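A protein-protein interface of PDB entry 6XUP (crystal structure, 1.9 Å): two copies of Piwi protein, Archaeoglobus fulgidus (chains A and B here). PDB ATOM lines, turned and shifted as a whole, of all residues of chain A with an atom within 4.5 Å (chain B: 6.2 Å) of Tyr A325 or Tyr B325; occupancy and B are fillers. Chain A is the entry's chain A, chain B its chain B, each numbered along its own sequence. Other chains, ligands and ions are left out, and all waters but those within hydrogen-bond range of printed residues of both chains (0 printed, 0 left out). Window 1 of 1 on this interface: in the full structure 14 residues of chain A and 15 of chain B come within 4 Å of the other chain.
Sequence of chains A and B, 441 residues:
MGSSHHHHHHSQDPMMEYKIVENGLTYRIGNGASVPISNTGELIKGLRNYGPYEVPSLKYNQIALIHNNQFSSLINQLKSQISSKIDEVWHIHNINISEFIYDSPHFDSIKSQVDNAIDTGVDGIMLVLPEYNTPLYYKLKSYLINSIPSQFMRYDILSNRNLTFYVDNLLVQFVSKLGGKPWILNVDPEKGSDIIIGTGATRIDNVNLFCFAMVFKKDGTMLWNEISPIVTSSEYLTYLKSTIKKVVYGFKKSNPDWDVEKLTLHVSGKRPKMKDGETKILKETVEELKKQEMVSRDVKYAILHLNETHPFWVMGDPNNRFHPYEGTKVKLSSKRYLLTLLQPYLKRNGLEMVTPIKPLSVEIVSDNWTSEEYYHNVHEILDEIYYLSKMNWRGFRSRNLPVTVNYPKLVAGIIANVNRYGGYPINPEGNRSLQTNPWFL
OH of Tyr A325 lies close to OG1 of Thr B328.
OG1 of Thr A340 sits at hydrogen-bond distance from O of Tyr A325 (3.0 Å).
The backbone NH of Thr A340 sits at hydrogen-bond distance from the backbone carbonyl oxygen of Thr A328.
The backbone carbonyl oxygen (O) of Tyr B325 is in hydrogen-bond range of the side-chain hydroxyl (OG1) of Thr B328 (3.1 Å).
O of Tyr B325 is in hydrogen-bond range of OG1 of Thr B340 (3.3 Å).
The backbone carbonyl oxygen (O) of Thr B328 sits close to the side-chain hydroxyl (OG1) of Thr B340 (3.4 Å).
Val A314 touches Lys B329.
CE2 of Tyr A325 touches CE2 of Tyr B325, 3.6 Å away.
Thr A328 touches Tyr B325 (CG2 to OH, 3.0 Å).
Of chain B, only Tyr B325 and Thr B328 come within 4 Å of Tyr A325.
Tyr B325 touches just these residues of chain A: Tyr A325 (3.6 Å) and Thr A328 (3.0 Å).
Of the printed residues of chain B, Val A314 touches Lys B329 (3.6 Å).
Of the printed residues of chain A, Lys B329 touches Val A314.
The nearest residue of chain B that does not touch Tyr A325 is Pro B324 (4.4 Å).
The nearest residue of chain A that does not touch Tyr B325 is Pro A324 (4.4 Å).
Of the 14 printed residues of chain B, 3 touch a printed residue of chain A.
Of the 8 printed residues of chain A, 3 touch a printed residue of chain B.
Hydrophobic or aromatic side chains of chain A that line the printed part of chain B: Val A314 and Tyr A325.
Along chain A the printed residues that touch a printed residue of chain B span positions 314 to 328.
Among the printed residues, 4 pairs touch across the chains.
Tyr B325 touches its own counterpart, Tyr A325.
Tyr A325 touches Thr B328, and with the chains exchanged Thr A328 touches Tyr B325.
Positions printed for both chains: 314, 324, 325, 326, 327, 328, 340 and 357.
Of the 4 pairs that touch across the chains among the printed residues, 3 have their exchanged pair printed and touching as well.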
ATOM      1  N   VAL A 314       4.142  10.764   0.365  1.00  0.00           N
ATOM      2  CA  VAL A 314       4.151  10.292  -1.015  1.00  0.00           C
ATOM      3  C   VAL A 314       5.529  10.575  -1.604  1.00  0.00           C
ATOM      4  O   VAL A 314       6.023  11.705  -1.539  1.00  0.00           O
ATOM      5  CB  VAL A 314       3.032  10.949  -1.833  1.00  0.00           C
ATOM      6  CG1 VAL A 314       3.077  10.483  -3.271  1.00  0.00           C
ATOM      7  CG2 VAL A 314       1.678  10.611  -1.226  1.00  0.00           C
ATOM      8  N   PRO A 324      -1.833  17.229  -6.605  1.00  0.00           N
ATOM      9  CA  PRO A 324      -2.241  15.896  -7.072  1.00  0.00           C
ATOM     10  C   PRO A 324      -3.053  15.130  -6.021  1.00  0.00           C
ATOM     11  O   PRO A 324      -3.946  14.356  -6.392  1.00  0.00           O
ATOM     12  CB  PRO A 324      -0.908  15.198  -7.353  1.00  0.00           C
ATOM     13  CG  PRO A 324       0.051  16.315  -7.627  1.00  0.00           C
ATOM     14  CD  PRO A 324      -0.382  17.445  -6.729  1.00  0.00           C
ATOM     15  N   TYR A 325      -2.750  15.356  -4.737  1.00  0.00           N
ATOM     16  CA  TYR A 325      -3.457  14.740  -3.614  1.00  0.00           C
ATOM     17  C   TYR A 325      -4.273  15.760  -2.828  1.00  0.00           C
ATOM     18  O   TYR A 325      -4.771  15.448  -1.738  1.00  0.00           O
ATOM     19  CB  TYR A 325      -2.468  14.016  -2.690  1.00  0.00           C
ATOM     20  CG  TYR A 325      -1.652  12.956  -3.414  1.00  0.00           C
ATOM     21  CD1 TYR A 325      -0.654  13.314  -4.319  1.00  0.00           C
ATOM     22  CD2 TYR A 325      -1.909  11.604  -3.228  1.00  0.00           C
ATOM     23  CE1 TYR A 325       0.075  12.364  -5.004  1.00  0.00           C
ATOM     24  CE2 TYR A 325      -1.177  10.639  -3.907  1.00  0.00           C
ATOM     25  CZ  TYR A 325      -0.184  11.030  -4.794  1.00  0.00           C
ATOM     26  OH  TYR A 325       0.554  10.090  -5.480  1.00  0.00           O
ATOM     27  N   GLU A 326      -4.419  16.967  -3.363  1.00  0.00           N
ATOM     28  CA  GLU A 326      -5.140  18.047  -2.705  1.00  0.00           C
ATOM     29  C   GLU A 326      -6.633  17.854  -2.939  1.00  0.00           C
ATOM     30  O   GLU A 326      -7.140  18.084  -4.046  1.00  0.00           O
ATOM     31  CB  GLU A 326      -4.648  19.393  -3.233  1.00  0.00           C
ATOM     32  CG  GLU A 326      -5.419  20.604  -2.726  1.00  0.00           C
ATOM     33  CD  GLU A 326      -5.123  20.953  -1.273  1.00  0.00           C
ATOM     34  OE1 GLU A 326      -4.084  20.505  -0.731  1.00  0.00           O
ATOM     35  OE2 GLU A 326      -5.940  21.691  -0.678  1.00  0.00           O
ATOM     36  N   GLY A 327      -7.338  17.429  -1.900  1.00  0.00           N
ATOM     37  CA  GLY A 327      -8.759  17.192  -2.013  1.00  0.00           C
ATOM     38  C   GLY A 327      -9.138  15.816  -2.501  1.00  0.00           C
ATOM     39  O   GLY A 327     -10.276  15.629  -2.953  1.00  0.00           O
ATOM     40  N   THR A 328      -8.227  14.845  -2.414  1.00  0.00           N
ATOM     41  CA  THR A 328      -8.463  13.458  -2.849  1.00  0.00           C
ATOM     42  C   THR A 328      -9.333  12.744  -1.819  1.00  0.00           C
ATOM     43  O   THR A 328      -9.037  12.796  -0.621  1.00  0.00           O
ATOM     44  CB  THR A 328      -7.126  12.741  -3.029  1.00  0.00           C
ATOM     45  OG1 THR A 328      -6.560  13.357  -4.178  1.00  0.00           O
ATOM     46  CG2 THR A 328      -7.270  11.257  -3.267  1.00  0.00           C
ATOM     47  N   THR A 340      -7.267  12.790   2.030  1.00  0.00           N
ATOM     48  CA  THR A 340      -5.813  12.973   2.096  1.00  0.00           C
ATOM     49  C   THR A 340      -5.556  14.466   2.165  1.00  0.00           C
ATOM     50  O   THR A 340      -5.462  15.146   1.146  1.00  0.00           O
ATOM     51  CB  THR A 340      -5.071  12.356   0.910  1.00  0.00           C
ATOM     52  OG1 THR A 340      -5.564  12.896  -0.312  1.00  0.00           O
ATOM     53  CG2 THR A 340      -5.181  10.858   0.893  1.00  0.00           C
ATOM     54  N   ILE A 357       1.439  13.827   4.020  1.00  0.00           N
ATOM     55  CA  ILE A 357      -0.017  13.737   4.010  1.00  0.00           C
ATOM     56  C   ILE A 357      -0.494  13.507   5.432  1.00  0.00           C
ATOM     57  O   ILE A 357       0.082  12.693   6.160  1.00  0.00           O
ATOM     58  CB  ILE A 357      -0.523  12.612   3.088  1.00  0.00           C
ATOM     59  CG1 ILE A 357       0.132  12.716   1.711  1.00  0.00           C
ATOM     60  CG2 ILE A 357      -2.048  12.663   2.982  1.00  0.00           C
ATOM     61  CD1 ILE A 357      -0.437  13.802   0.862  1.00  0.00           C
ATOM     62  N   PHE B 312      -8.871  -0.267  -1.977  1.00  0.00           N
ATOM     63  CA  PHE B 312      -9.675   0.934  -1.834  1.00  0.00           C
ATOM     64  C   PHE B 312      -9.922   1.541  -3.198  1.00  0.00           C
ATOM     65  O   PHE B 312      -9.361   1.107  -4.207  1.00  0.00           O
ATOM     66  CB  PHE B 312      -9.040   1.972  -0.886  1.00  0.00           C
ATOM     67  CG  PHE B 312      -7.649   2.404  -1.250  1.00  0.00           C
ATOM     68  CD1 PHE B 312      -7.423   3.416  -2.166  1.00  0.00           C
ATOM     69  CD2 PHE B 312      -6.556   1.820  -0.625  1.00  0.00           C
ATOM     70  CE1 PHE B 312      -6.138   3.818  -2.465  1.00  0.00           C
ATOM     71  CE2 PHE B 312      -5.282   2.226  -0.916  1.00  0.00           C
ATOM     72  CZ  PHE B 312      -5.065   3.217  -1.837  1.00  0.00           C
ATOM     73  N   VAL B 314     -10.241   5.344  -5.229  1.00  0.00           N
ATOM     74  CA  VAL B 314     -10.119   6.796  -5.267  1.00  0.00           C
ATOM     75  C   VAL B 314     -11.354   7.346  -5.971  1.00  0.00           C
ATOM     76  O   VAL B 314     -11.671   6.930  -7.089  1.00  0.00           O
ATOM     77  CB  VAL B 314      -8.839   7.235  -5.984  1.00  0.00           C
ATOM     78  CG1 VAL B 314      -8.828   8.752  -6.153  1.00  0.00           C
ATOM     79  CG2 VAL B 314      -7.608   6.743  -5.262  1.00  0.00           C
ATOM     80  N   PRO B 324      -3.280   8.899 -12.383  1.00  0.00           N
ATOM     81  CA  PRO B 324      -2.533   9.806 -11.512  1.00  0.00           C
ATOM     82  C   PRO B 324      -1.862   9.057 -10.358  1.00  0.00           C
ATOM     83  O   PRO B 324      -1.139   9.654  -9.553  1.00  0.00           O
ATOM     84  CB  PRO B 324      -3.453  10.901 -10.972  1.00  0.00           C
ATOM     85  N   TYR B 325      -2.102   7.743 -10.288  1.00  0.00           N
ATOM     86  CA  TYR B 325      -1.549   6.900  -9.235  1.00  0.00           C
ATOM     87  C   TYR B 325      -0.638   5.793  -9.747  1.00  0.00           C
ATOM     88  O   TYR B 325      -0.062   5.065  -8.931  1.00  0.00           O
ATOM     89  CB  TYR B 325      -2.684   6.289  -8.397  1.00  0.00           C
ATOM     90  CG  TYR B 325      -3.372   7.323  -7.555  1.00  0.00           C
ATOM     91  CD1 TYR B 325      -4.411   8.091  -8.077  1.00  0.00           C
ATOM     92  CD2 TYR B 325      -2.955   7.573  -6.253  1.00  0.00           C
ATOM     93  CE1 TYR B 325      -5.034   9.063  -7.321  1.00  0.00           C
ATOM     94  CE2 TYR B 325      -3.574   8.542  -5.480  1.00  0.00           C
ATOM     95  CZ  TYR B 325      -4.614   9.283  -6.020  1.00  0.00           C
ATOM     96  OH  TYR B 325      -5.233  10.250  -5.262  1.00  0.00           O
ATOM     97  N   GLU B 326      -0.484   5.641 -11.062  1.00  0.00           N
ATOM     98  CA  GLU B 326       0.355   4.575 -11.596  1.00  0.00           C
ATOM     99  C   GLU B 326       1.812   4.826 -11.237  1.00  0.00           C
ATOM    100  O   GLU B 326       2.398   5.839 -11.634  1.00  0.00           O
ATOM    101  CB  GLU B 326       0.187   4.450 -13.108  1.00  0.00           C
ATOM    102  CG  GLU B 326      -0.918   3.478 -13.525  1.00  0.00           C
ATOM    103  CD  GLU B 326      -0.381   2.109 -13.961  1.00  0.00           C
ATOM    104  OE1 GLU B 326      -1.172   1.135 -13.985  1.00  0.00           O
ATOM    105  OE2 GLU B 326       0.832   1.999 -14.257  1.00  0.00           O
ATOM    106  N   GLY B 327       2.397   3.896 -10.491  1.00  0.00           N
ATOM    107  CA  GLY B 327       3.768   4.031 -10.064  1.00  0.00           C
ATOM    108  C   GLY B 327       3.956   4.799  -8.780  1.00  0.00           C
ATOM    109  O   GLY B 327       5.105   5.074  -8.408  1.00  0.00           O
ATOM    110  N   THR B 328       2.872   5.131  -8.082  1.00  0.00           N
ATOM    111  CA  THR B 328       2.958   5.951  -6.883  1.00  0.00           C
ATOM    112  C   THR B 328       3.475   5.137  -5.701  1.00  0.00           C
ATOM    113  O   THR B 328       2.962   4.053  -5.402  1.00  0.00           O
ATOM    114  CB  THR B 328       1.596   6.555  -6.557  1.00  0.00           C
ATOM    115  OG1 THR B 328       1.264   7.523  -7.552  1.00  0.00           O
ATOM    116  CG2 THR B 328       1.633   7.232  -5.202  1.00  0.00           C
ATOM    117  N   LYS B 329       4.497   5.666  -5.038  1.00  0.00           N
ATOM    118  CA  LYS B 329       5.099   5.056  -3.863  1.00  0.00           C
ATOM    119  C   LYS B 329       4.758   5.893  -2.641  1.00  0.00           C
ATOM    120  O   LYS B 329       4.874   7.123  -2.669  1.00  0.00           O
ATOM    121  CB  LYS B 329       6.620   4.943  -4.010  1.00  0.00           C
ATOM    122  CG  LYS B 329       7.092   4.393  -5.353  1.00  0.00           C
ATOM    123  CD  LYS B 329       8.614   4.423  -5.423  1.00  0.00           C
ATOM    124  CE  LYS B 329       9.095   4.822  -6.810  1.00  0.00           C
ATOM    125  NZ  LYS B 329       8.519   6.126  -7.245  1.00  0.00           N
ATOM    126  N   VAL B 330       4.344   5.222  -1.574  1.00  0.00           N
ATOM    127  CA  VAL B 330       3.981   5.859  -0.318  1.00  0.00           C
ATOM    128  C   VAL B 330       4.940   5.364   0.754  1.00  0.00           C
ATOM    129  O   VAL B 330       5.206   4.159   0.858  1.00  0.00           O
ATOM    130  CB  VAL B 330       2.518   5.566   0.059  1.00  0.00           C
ATOM    131  CG1 VAL B 330       2.247   6.008   1.464  1.00  0.00           C
ATOM    132  CG2 VAL B 330       1.593   6.259  -0.907  1.00  0.00           C
ATOM    133  N   THR B 340       0.637   1.790  -4.504  1.00  0.00           N
ATOM    134  CA  THR B 340      -0.747   1.856  -4.956  1.00  0.00           C
ATOM    135  C   THR B 340      -0.801   1.271  -6.358  1.00  0.00           C
ATOM    136  O   THR B 340      -0.707   1.987  -7.356  1.00  0.00           O
ATOM    137  CB  THR B 340      -1.243   3.297  -4.950  1.00  0.00           C
ATOM    138  OG1 THR B 340      -0.376   4.095  -5.769  1.00  0.00           O
ATOM    139  CG2 THR B 340      -1.261   3.860  -3.544  1.00  0.00           C
ATOM    140  N   LEU B 341      -0.980  -0.044  -6.435  1.00  0.00           N
ATOM    141  CA  LEU B 341      -1.051  -0.742  -7.713  1.00  0.00           C
ATOM    142  C   LEU B 341      -2.446  -0.579  -8.308  1.00  0.00           C
ATOM    143  O   LEU B 341      -3.437  -0.990  -7.692  1.00  0.00           O
ATOM    144  CB  LEU B 341      -0.707  -2.222  -7.521  1.00  0.00           C
ATOM    145  CG  LEU B 341       0.680  -2.474  -6.917  1.00  0.00           C
ATOM    146  CD1 LEU B 341       0.984  -3.968  -6.605  1.00  0.00           C
ATOM    147  CD2 LEU B 341       1.744  -1.884  -7.812  1.00  0.00           C
ATOM    148  N   LEU B 342      -2.529   0.018  -9.497  1.00  0.00           N
ATOM    149  CA  LEU B 342      -3.815   0.152 -10.174  1.00  0.00           C
ATOM    150  C   LEU B 342      -4.201  -1.140 -10.878  1.00  0.00           C
ATOM    151  O   LEU B 342      -3.355  -1.850 -11.432  1.00  0.00           O
ATOM    152  CB  LEU B 342      -3.793   1.279 -11.203  1.00  0.00           C
ATOM    153  CG  LEU B 342      -3.996   2.680 -10.651  1.00  0.00           C
ATOM    154  CD1 LEU B 342      -2.654   3.214 -10.230  1.00  0.00           C
ATOM    155  CD2 LEU B 342      -4.650   3.598 -11.678  1.00  0.00           C
ATOM    156  N   THR B 355     -11.542   4.830  -9.049  1.00  0.00           N
ATOM    157  CA  THR B 355     -10.286   4.207  -9.465  1.00  0.00           C
ATOM    158  C   THR B 355      -9.931   3.143  -8.436  1.00  0.00           C
ATOM    159  O   THR B 355      -9.454   3.473  -7.335  1.00  0.00           O
ATOM    160  CB  THR B 355      -9.158   5.227  -9.583  1.00  0.00           C
ATOM    161  OG1 THR B 355      -9.485   6.211 -10.570  1.00  0.00           O
ATOM    162  CG2 THR B 355      -7.856   4.537  -9.970  1.00  0.00           C
ATOM    163  N   ILE B 357      -7.886   0.546  -6.355  1.00  0.00           N
ATOM    164  CA  ILE B 357      -6.481   0.410  -6.002  1.00  0.00           C
ATOM    165  C   ILE B 357      -6.313  -0.884  -5.220  1.00  0.00           C
ATOM    166  O   ILE B 357      -7.082  -1.153  -4.290  1.00  0.00           O
ATOM    167  CB  ILE B 357      -5.991   1.618  -5.181  1.00  0.00           C
ATOM    168  CG1 ILE B 357      -6.265   2.916  -5.940  1.00  0.00           C
ATOM    169  CG2 ILE B 357      -4.515   1.505  -4.876  1.00  0.00           C
ATOM    170  CD1 ILE B 357      -5.387   3.096  -7.149  1.00  0.00           C
